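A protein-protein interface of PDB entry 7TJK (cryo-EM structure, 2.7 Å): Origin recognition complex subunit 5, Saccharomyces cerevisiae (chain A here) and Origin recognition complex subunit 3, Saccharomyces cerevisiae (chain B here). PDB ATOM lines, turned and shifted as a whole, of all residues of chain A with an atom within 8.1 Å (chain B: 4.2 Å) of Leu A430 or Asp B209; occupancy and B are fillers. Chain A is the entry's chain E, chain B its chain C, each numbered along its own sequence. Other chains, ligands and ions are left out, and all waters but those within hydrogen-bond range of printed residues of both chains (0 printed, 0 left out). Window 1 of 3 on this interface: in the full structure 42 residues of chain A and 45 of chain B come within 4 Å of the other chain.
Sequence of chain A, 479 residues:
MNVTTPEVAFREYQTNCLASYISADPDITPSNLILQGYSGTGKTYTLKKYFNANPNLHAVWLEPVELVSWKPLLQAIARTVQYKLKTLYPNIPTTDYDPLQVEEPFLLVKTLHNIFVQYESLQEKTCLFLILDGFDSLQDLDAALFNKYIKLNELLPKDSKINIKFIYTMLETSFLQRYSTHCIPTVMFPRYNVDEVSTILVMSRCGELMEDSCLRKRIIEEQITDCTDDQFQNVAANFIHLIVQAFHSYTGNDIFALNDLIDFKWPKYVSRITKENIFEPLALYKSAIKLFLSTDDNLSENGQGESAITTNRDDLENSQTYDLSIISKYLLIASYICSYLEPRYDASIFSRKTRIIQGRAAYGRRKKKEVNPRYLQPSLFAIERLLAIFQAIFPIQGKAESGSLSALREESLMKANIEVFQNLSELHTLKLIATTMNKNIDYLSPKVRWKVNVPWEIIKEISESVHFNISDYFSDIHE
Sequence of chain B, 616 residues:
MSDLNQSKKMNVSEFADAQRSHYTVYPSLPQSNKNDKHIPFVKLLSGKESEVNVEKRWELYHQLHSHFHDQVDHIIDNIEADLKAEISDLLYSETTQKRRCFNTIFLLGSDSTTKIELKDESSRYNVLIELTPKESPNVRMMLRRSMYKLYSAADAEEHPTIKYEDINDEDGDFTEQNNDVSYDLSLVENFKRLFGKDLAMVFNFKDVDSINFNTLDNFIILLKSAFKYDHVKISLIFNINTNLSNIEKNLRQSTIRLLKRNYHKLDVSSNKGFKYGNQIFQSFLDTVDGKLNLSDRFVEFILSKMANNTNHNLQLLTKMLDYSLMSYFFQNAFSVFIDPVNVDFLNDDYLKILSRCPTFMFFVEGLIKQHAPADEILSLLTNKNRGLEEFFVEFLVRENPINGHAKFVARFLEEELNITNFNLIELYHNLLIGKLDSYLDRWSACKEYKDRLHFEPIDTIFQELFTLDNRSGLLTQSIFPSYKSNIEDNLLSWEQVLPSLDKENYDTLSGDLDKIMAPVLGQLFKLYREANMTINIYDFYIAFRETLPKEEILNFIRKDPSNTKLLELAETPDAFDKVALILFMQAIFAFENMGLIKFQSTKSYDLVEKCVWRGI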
ATOM      1  N   LEU A 324     -11.602  -6.562 -14.734  1.00  0.00           N
ATOM      2  CA  LEU A 324     -10.170  -6.472 -14.464  1.00  0.00           C
ATOM      3  C   LEU A 324      -9.831  -7.080 -13.111  1.00  0.00           C
ATOM      4  O   LEU A 324     -10.701  -7.257 -12.260  1.00  0.00           O
ATOM      5  CB  LEU A 324      -9.680  -5.018 -14.513  1.00  0.00           C
ATOM      6  CG  LEU A 324      -9.439  -4.294 -15.844  1.00  0.00           C
ATOM      7  CD1 LEU A 324     -10.722  -3.940 -16.595  1.00  0.00           C
ATOM      8  CD2 LEU A 324      -8.590  -3.048 -15.615  1.00  0.00           C
ATOM      9  N   SER A 328      -4.653  -4.955 -11.832  1.00  0.00           N
ATOM     10  CA  SER A 328      -4.917  -4.078 -12.971  1.00  0.00           C
ATOM     11  C   SER A 328      -5.709  -2.841 -12.561  1.00  0.00           C
ATOM     12  O   SER A 328      -5.431  -1.735 -13.041  1.00  0.00           O
ATOM     13  CB  SER A 328      -5.663  -4.846 -14.062  1.00  0.00           C
ATOM     14  OG  SER A 328      -4.837  -5.830 -14.658  1.00  0.00           O
ATOM     15  N   LEU A 332      -4.339   0.948 -12.781  1.00  0.00           N
ATOM     16  CA  LEU A 332      -5.056   2.018 -13.474  1.00  0.00           C
ATOM     17  C   LEU A 332      -5.298   3.213 -12.557  1.00  0.00           C
ATOM     18  O   LEU A 332      -5.169   4.372 -12.987  1.00  0.00           O
ATOM     19  CB  LEU A 332      -6.376   1.478 -14.024  1.00  0.00           C
ATOM     20  CG  LEU A 332      -6.986   2.153 -15.255  1.00  0.00           C
ATOM     21  CD1 LEU A 332      -5.930   2.408 -16.304  1.00  0.00           C
ATOM     22  CD2 LEU A 332      -8.098   1.296 -15.833  1.00  0.00           C
ATOM     23  N   ASN A 423       0.127  -7.533 -16.059  1.00  0.00           N
ATOM     24  CA  ASN A 423      -1.109  -6.758 -16.007  1.00  0.00           C
ATOM     25  C   ASN A 423      -0.931  -5.377 -16.628  1.00  0.00           C
ATOM     26  O   ASN A 423      -1.848  -4.862 -17.276  1.00  0.00           O
ATOM     27  CB  ASN A 423      -1.585  -6.640 -14.563  1.00  0.00           C
ATOM     28  CG  ASN A 423      -2.371  -7.851 -14.111  1.00  0.00           C
ATOM     29  OD1 ASN A 423      -3.440  -8.146 -14.643  1.00  0.00           O
ATOM     30  ND2 ASN A 423      -1.846  -8.560 -13.120  1.00  0.00           N
ATOM     31  N   LEU A 424       0.243  -4.766 -16.441  1.00  0.00           N
ATOM     32  CA  LEU A 424       0.514  -3.470 -17.055  1.00  0.00           C
ATOM     33  C   LEU A 424       0.604  -3.577 -18.575  1.00  0.00           C
ATOM     34  O   LEU A 424       0.098  -2.707 -19.300  1.00  0.00           O
ATOM     35  CB  LEU A 424       1.800  -2.886 -16.474  1.00  0.00           C
ATOM     36  CG  LEU A 424       2.184  -1.459 -16.864  1.00  0.00           C
ATOM     37  CD1 LEU A 424       1.005  -0.509 -16.732  1.00  0.00           C
ATOM     38  CD2 LEU A 424       3.345  -0.995 -16.008  1.00  0.00           C
ATOM     39  N   SER A 425       1.240  -4.643 -19.073  1.00  0.00           N
ATOM     40  CA  SER A 425       1.283  -4.896 -20.510  1.00  0.00           C
ATOM     41  C   SER A 425      -0.109  -5.161 -21.067  1.00  0.00           C
ATOM     42  O   SER A 425      -0.422  -4.753 -22.191  1.00  0.00           O
ATOM     43  CB  SER A 425       2.205  -6.078 -20.802  1.00  0.00           C
ATOM     44  OG  SER A 425       3.443  -5.933 -20.139  1.00  0.00           O
ATOM     45  N   GLU A 426      -0.954  -5.848 -20.291  1.00  0.00           N
ATOM     46  CA  GLU A 426      -2.342  -6.049 -20.697  1.00  0.00           C
ATOM     47  C   GLU A 426      -3.110  -4.734 -20.738  1.00  0.00           C
ATOM     48  O   GLU A 426      -3.945  -4.530 -21.624  1.00  0.00           O
ATOM     49  CB  GLU A 426      -3.029  -7.037 -19.754  1.00  0.00           C
ATOM     50  CG  GLU A 426      -4.366  -7.564 -20.259  1.00  0.00           C
ATOM     51  CD  GLU A 426      -4.350  -7.949 -21.729  1.00  0.00           C
ATOM     52  OE1 GLU A 426      -3.473  -8.740 -22.141  1.00  0.00           O
ATOM     53  OE2 GLU A 426      -5.255  -7.504 -22.467  1.00  0.00           O
ATOM     54  N   LEU A 427      -2.847  -3.842 -19.776  1.00  0.00           N
ATOM     55  CA  LEU A 427      -3.478  -2.524 -19.765  1.00  0.00           C
ATOM     56  C   LEU A 427      -3.072  -1.705 -20.982  1.00  0.00           C
ATOM     57  O   LEU A 427      -3.895  -0.981 -21.555  1.00  0.00           O
ATOM     58  CB  LEU A 427      -3.118  -1.778 -18.480  1.00  0.00           C
ATOM     59  CG  LEU A 427      -3.887  -2.121 -17.202  1.00  0.00           C
ATOM     60  CD1 LEU A 427      -3.400  -1.266 -16.044  1.00  0.00           C
ATOM     61  CD2 LEU A 427      -5.381  -1.951 -17.402  1.00  0.00           C
ATOM     62  N   HIS A 428      -1.803  -1.804 -21.389  1.00  0.00           N
ATOM     63  CA  HIS A 428      -1.387  -1.163 -22.635  1.00  0.00           C
ATOM     64  C   HIS A 428      -2.015  -1.841 -23.850  1.00  0.00           C
ATOM     65  O   HIS A 428      -2.268  -1.175 -24.861  1.00  0.00           O
ATOM     66  CB  HIS A 428       0.144  -1.143 -22.739  1.00  0.00           C
ATOM     67  CG  HIS A 428       0.676  -0.325 -23.883  1.00  0.00           C
ATOM     68  ND1 HIS A 428       0.496  -0.670 -25.206  1.00  0.00           N
ATOM     69  CD2 HIS A 428       1.363   0.841 -23.895  1.00  0.00           C
ATOM     70  CE1 HIS A 428       1.062   0.239 -25.980  1.00  0.00           C
ATOM     71  NE2 HIS A 428       1.594   1.168 -25.208  1.00  0.00           N
ATOM     72  N   THR A 429      -2.260  -3.152 -23.782  1.00  0.00           N
ATOM     73  CA  THR A 429      -2.926  -3.843 -24.883  1.00  0.00           C
ATOM     74  C   THR A 429      -4.386  -3.409 -25.001  1.00  0.00           C
ATOM     75  O   THR A 429      -4.903  -3.226 -26.111  1.00  0.00           O
ATOM     76  CB  THR A 429      -2.812  -5.358 -24.685  1.00  0.00           C
ATOM     77  OG1 THR A 429      -1.429  -5.727 -24.644  1.00  0.00           O
ATOM     78  CG2 THR A 429      -3.481  -6.122 -25.818  1.00  0.00           C
ATOM     79  N   LEU A 430      -5.048  -3.179 -23.867  1.00  0.00           N
ATOM     80  CA  LEU A 430      -6.446  -2.763 -23.833  1.00  0.00           C
ATOM     81  C   LEU A 430      -6.654  -1.298 -24.205  1.00  0.00           C
ATOM     82  O   LEU A 430      -7.811  -0.857 -24.208  1.00  0.00           O
ATOM     83  CB  LEU A 430      -7.027  -3.014 -22.442  1.00  0.00           C
ATOM     84  CG  LEU A 430      -7.201  -4.475 -22.026  1.00  0.00           C
ATOM     85  CD1 LEU A 430      -7.304  -4.591 -20.515  1.00  0.00           C
ATOM     86  CD2 LEU A 430      -8.401  -5.087 -22.706  1.00  0.00           C
ATOM     87  N   LYS A 431      -5.573  -0.557 -24.487  1.00  0.00           N
ATOM     88  CA  LYS A 431      -5.575   0.884 -24.773  1.00  0.00           C
ATOM     89  C   LYS A 431      -6.159   1.696 -23.620  1.00  0.00           C
ATOM     90  O   LYS A 431      -6.748   2.758 -23.830  1.00  0.00           O
ATOM     91  CB  LYS A 431      -6.292   1.214 -26.089  1.00  0.00           C
ATOM     92  CG  LYS A 431      -5.709   0.518 -27.303  1.00  0.00           C
ATOM     93  CD  LYS A 431      -4.488   1.249 -27.829  1.00  0.00           C
ATOM     94  CE  LYS A 431      -3.556   0.305 -28.574  1.00  0.00           C
ATOM     95  NZ  LYS A 431      -3.311  -0.952 -27.814  1.00  0.00           N
ATOM     96  N   LEU A 432      -6.000   1.198 -22.395  1.00  0.00           N
ATOM     97  CA  LEU A 432      -6.310   1.974 -21.205  1.00  0.00           C
ATOM     98  C   LEU A 432      -5.104   2.751 -20.702  1.00  0.00           C
ATOM     99  O   LEU A 432      -5.267   3.695 -19.924  1.00  0.00           O
ATOM    100  CB  LEU A 432      -6.834   1.057 -20.094  1.00  0.00           C
ATOM    101  CG  LEU A 432      -7.989   0.108 -20.437  1.00  0.00           C
ATOM    102  CD1 LEU A 432      -8.485  -0.611 -19.191  1.00  0.00           C
ATOM    103  CD2 LEU A 432      -9.140   0.820 -21.133  1.00  0.00           C
ATOM    104  N   ILE A 433      -3.903   2.362 -21.129  1.00  0.00           N
ATOM    105  CA  ILE A 433      -2.673   3.114 -20.918  1.00  0.00           C
ATOM    106  C   ILE A 433      -2.072   3.402 -22.285  1.00  0.00           C
ATOM    107  O   ILE A 433      -1.953   2.500 -23.120  1.00  0.00           O
ATOM    108  CB  ILE A 433      -1.666   2.346 -20.036  1.00  0.00           C
ATOM    109  CG1 ILE A 433      -2.316   1.907 -18.728  1.00  0.00           C
ATOM    110  CG2 ILE A 433      -0.430   3.193 -19.756  1.00  0.00           C
ATOM    111  CD1 ILE A 433      -2.617   3.046 -17.813  1.00  0.00           C
ATOM    112  N   ALA A 434      -1.699   4.657 -22.515  1.00  0.00           N
ATOM    113  CA  ALA A 434      -1.111   5.065 -23.778  1.00  0.00           C
ATOM    114  C   ALA A 434       0.328   5.513 -23.569  1.00  0.00           C
ATOM    115  O   ALA A 434       0.739   5.888 -22.468  1.00  0.00           O
ATOM    116  CB  ALA A 434      -1.920   6.193 -24.436  1.00  0.00           C
ATOM    117  N   TYR A 443       9.099  -0.983 -25.377  1.00  0.00           N
ATOM    118  CA  TYR A 443       8.619  -0.849 -24.008  1.00  0.00           C
ATOM    119  C   TYR A 443       9.743  -0.590 -23.017  1.00  0.00           C
ATOM    120  O   TYR A 443       9.490  -0.035 -21.943  1.00  0.00           O
ATOM    121  CB  TYR A 443       7.865  -2.112 -23.593  1.00  0.00           C
ATOM    122  CG  TYR A 443       6.472  -2.227 -24.167  1.00  0.00           C
ATOM    123  CD1 TYR A 443       5.492  -1.295 -23.853  1.00  0.00           C
ATOM    124  CD2 TYR A 443       6.134  -3.277 -25.015  1.00  0.00           C
ATOM    125  CE1 TYR A 443       4.216  -1.399 -24.372  1.00  0.00           C
ATOM    126  CE2 TYR A 443       4.860  -3.391 -25.539  1.00  0.00           C
ATOM    127  CZ  TYR A 443       3.907  -2.450 -25.214  1.00  0.00           C
ATOM    128  OH  TYR A 443       2.637  -2.558 -25.732  1.00  0.00           O
ATOM    129  N   ASN A 453      -5.434   6.622 -20.247  1.00  0.00           N
ATOM    130  CA  ASN A 453      -6.220   6.842 -21.453  1.00  0.00           C
ATOM    131  C   ASN A 453      -7.709   6.846 -21.139  1.00  0.00           C
ATOM    132  O   ASN A 453      -8.547   7.029 -22.026  1.00  0.00           O
ATOM    133  CB  ASN A 453      -5.897   5.789 -22.512  1.00  0.00           C
ATOM    134  CG  ASN A 453      -6.084   6.306 -23.927  1.00  0.00           C
ATOM    135  OD1 ASN A 453      -6.342   7.490 -24.139  1.00  0.00           O
ATOM    136  ND2 ASN A 453      -5.958   5.416 -24.902  1.00  0.00           N
ATOM    137  N   VAL A 454      -8.068   6.652 -19.873  1.00  0.00           N
ATOM    138  CA  VAL A 454      -9.481   6.605 -19.501  1.00  0.00           C
ATOM    139  C   VAL A 454      -9.878   7.889 -18.774  1.00  0.00           C
ATOM    140  O   VAL A 454      -9.037   8.522 -18.118  1.00  0.00           O
ATOM    141  CB  VAL A 454      -9.797   5.349 -18.669  1.00  0.00           C
ATOM    142  CG1 VAL A 454      -9.379   4.110 -19.428  1.00  0.00           C
ATOM    143  CG2 VAL A 454      -9.115   5.382 -17.315  1.00  0.00           C
ATOM    144  N   ASP B 207     -10.505  -7.782 -31.601  1.00  0.00           N
ATOM    145  CA  ASP B 207      -9.831  -6.830 -30.714  1.00  0.00           C
ATOM    146  C   ASP B 207     -10.299  -5.391 -30.907  1.00  0.00           C
ATOM    147  O   ASP B 207      -9.516  -4.537 -31.335  1.00  0.00           O
ATOM    148  CB  ASP B 207      -8.312  -6.910 -30.907  1.00  0.00           C
ATOM    149  CG  ASP B 207      -7.728  -8.209 -30.405  1.00  0.00           C
ATOM    150  OD1 ASP B 207      -8.296  -8.795 -29.460  1.00  0.00           O
ATOM    151  OD2 ASP B 207      -6.699  -8.648 -30.957  1.00  0.00           O
ATOM    152  N   VAL B 208     -11.572  -5.119 -30.601  1.00  0.00           N
ATOM    153  CA  VAL B 208     -12.165  -3.813 -30.874  1.00  0.00           C
ATOM    154  C   VAL B 208     -11.583  -2.723 -29.976  1.00  0.00           C
ATOM    155  O   VAL B 208     -11.553  -1.549 -30.367  1.00  0.00           O
ATOM    156  CB  VAL B 208     -13.698  -3.914 -30.734  1.00  0.00           C
ATOM    157  CG1 VAL B 208     -14.406  -2.688 -31.302  1.00  0.00           C
ATOM    158  CG2 VAL B 208     -14.200  -5.156 -31.424  1.00  0.00           C
ATOM    159  N   ASP B 209     -11.083  -3.085 -28.792  1.00  0.00           N
ATOM    160  CA  ASP B 209     -10.502  -2.104 -27.881  1.00  0.00           C
ATOM    161  C   ASP B 209      -9.213  -1.490 -28.417  1.00  0.00           C
ATOM    162  O   ASP B 209      -8.862  -0.374 -28.018  1.00  0.00           O
ATOM    163  CB  ASP B 209     -10.245  -2.748 -26.518  1.00  0.00           C
ATOM    164  CG  ASP B 209     -11.526  -3.087 -25.784  1.00  0.00           C
ATOM    165  OD1 ASP B 209     -12.539  -2.389 -25.998  1.00  0.00           O
ATOM    166  OD2 ASP B 209     -11.524  -4.053 -24.993  1.00  0.00           O
ATOM    167  N   SER B 210      -8.511  -2.181 -29.317  1.00  0.00           N
ATOM    168  CA  SER B 210      -7.271  -1.687 -29.897  1.00  0.00           C
ATOM    169  C   SER B 210      -7.458  -0.981 -31.235  1.00  0.00           C
ATOM    170  O   SER B 210      -6.487  -0.422 -31.757  1.00  0.00           O
ATOM    171  CB  SER B 210      -6.278  -2.842 -30.078  1.00  0.00           C
ATOM    172  OG  SER B 210      -4.989  -2.359 -30.409  1.00  0.00           O
ATOM    173  N   ILE B 211      -8.659  -0.987 -31.800  1.00  0.00           N
ATOM    174  CA  ILE B 211      -8.879  -0.371 -33.104  1.00  0.00           C
ATOM    175  C   ILE B 211      -9.025   1.137 -32.931  1.00  0.00           C
ATOM    176  O   ILE B 211      -9.314   1.639 -31.837  1.00  0.00           O
ATOM    177  CB  ILE B 211     -10.107  -0.994 -33.809  1.00  0.00           C
ATOM    178  CG1 ILE B 211      -9.940  -0.958 -35.330  1.00  0.00           C
ATOM    179  CG2 ILE B 211     -11.402  -0.287 -33.427  1.00  0.00           C
ATOM    180  CD1 ILE B 211     -11.033  -1.678 -36.083  1.00  0.00           C
ATOM    181  N   ILE B 240     -15.436  -7.419 -27.431  1.00  0.00           N
ATOM    182  CA  ILE B 240     -15.082  -6.392 -26.461  1.00  0.00           C
ATOM    183  C   ILE B 240     -14.406  -7.052 -25.270  1.00  0.00           C
ATOM    184  O   ILE B 240     -14.912  -8.043 -24.730  1.00  0.00           O
ATOM    185  CB  ILE B 240     -16.326  -5.605 -26.016  1.00  0.00           C
ATOM    186  CG1 ILE B 240     -17.161  -5.187 -27.227  1.00  0.00           C
ATOM    187  CG2 ILE B 240     -15.925  -4.393 -25.187  1.00  0.00           C
ATOM    188  CD1 ILE B 240     -16.441  -4.265 -28.179  1.00  0.00           C
ATOM    189  N   ASN B 241     -13.264  -6.507 -24.856  1.00  0.00           N
ATOM    190  CA  ASN B 241     -12.537  -7.037 -23.713  1.00  0.00           C
ATOM    191  C   ASN B 241     -12.612  -6.173 -22.463  1.00  0.00           C
ATOM    192  O   ASN B 241     -12.216  -6.646 -21.394  1.00  0.00           O
ATOM    193  CB  ASN B 241     -11.061  -7.259 -24.068  1.00  0.00           C
ATOM    194  CG  ASN B 241     -10.782  -8.669 -24.537  1.00  0.00           C
ATOM    195  OD1 ASN B 241     -11.198  -9.640 -23.904  1.00  0.00           O
ATOM    196  ND2 ASN B 241     -10.065  -8.792 -25.647  1.00  0.00           N
ATOM    197  N   THR B 242     -13.092  -4.932 -22.548  1.00  0.00           N
ATOM    198  CA  THR B 242     -13.128  -4.142 -21.324  1.00  0.00           C
ATOM    199  C   THR B 242     -14.518  -4.112 -20.704  1.00  0.00           C
ATOM    200  O   THR B 242     -14.739  -4.761 -19.675  1.00  0.00           O
ATOM    201  CB  THR B 242     -12.662  -2.711 -21.602  1.00  0.00           C
ATOM    202  OG1 THR B 242     -13.374  -2.186 -22.729  1.00  0.00           O
ATOM    203  CG2 THR B 242     -11.177  -2.684 -21.896  1.00  0.00           C
ATOM    204  N   ILE B 247     -16.824   1.549 -25.071  1.00  0.00           N
ATOM    205  CA  ILE B 247     -17.090   1.632 -26.502  1.00  0.00           C
ATOM    206  C   ILE B 247     -18.300   2.497 -26.840  1.00  0.00           C
ATOM    207  O   ILE B 247     -18.439   2.916 -27.998  1.00  0.00           O
ATOM    208  CB  ILE B 247     -17.269   0.238 -27.135  1.00  0.00           C
ATOM    209  CG1 ILE B 247     -18.570  -0.414 -26.677  1.00  0.00           C
ATOM    210  CG2 ILE B 247     -16.084  -0.652 -26.797  1.00  0.00           C
ATOM    211  CD1 ILE B 247     -18.984  -1.602 -27.504  1.00  0.00           C
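The side-chain hydroxyl (OG) of Ser B210 lies within hydrogen-bond range of the side-chain amino group (NZ) of Lys A431.
O of Thr A429 lies within hydrogen-bond range of NZ of Lys A431.
The backbone NH of Thr B242 is in hydrogen-bond range of the side-chain carboxylate of Asp B209 (3.0 Å).
The backbone carbonyl oxygen of Lys A431 is in hydrogen-bond range of the side-chain amide nitrogen of Asn A453 (3.0 Å).
The backbone NH of Asn B241 is in hydrogen-bond range of the side-chain carboxylate of Asp B209 (3.0 Å).
O of His A428 sits at hydrogen-bond distance from NZ of Lys A431, at 3.1 Å.
Among the printed residues, merely in contact across the chains: Leu A430 with Asp B209, Leu A430 with Asn B241, Leu A430 with Thr B242 and Lys A431 with Asp B209.
Leu A430 touches three residues of chain B.
Of the printed residues of chain A, Asn B241 touches Leu A430 (3.7 Å).
Printed residues of chain B within 4 Å of Lys A431: Asp B209 and Ser B210.
Printed residues of chain A within 4 Å of Thr B242: Leu A430.
Printed residues of chain A within 4 Å of Ser B210: Lys A431 (3.4 Å).
Val A454 touches none of the printed residues of chain B.
Val B208 touches none of the printed residues of chain A.
The nearest printed residue of chain B that does not touch Leu A430 is Ser B210 (5.3 Å).
The nearest printed residue of chain A that does not touch Asn B241 is Leu A324 (5.7 Å).
Hydrophobic or aromatic side chains of chain A within 4 Å of the printed part of chain B: Leu A430.
Among the printed residues, 5 pairs touch across the chains.
Among the printed residues, no Asp or Glu carboxylate lies within 4 Å of a Lys or Arg side-chain nitrogen of the other chain.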
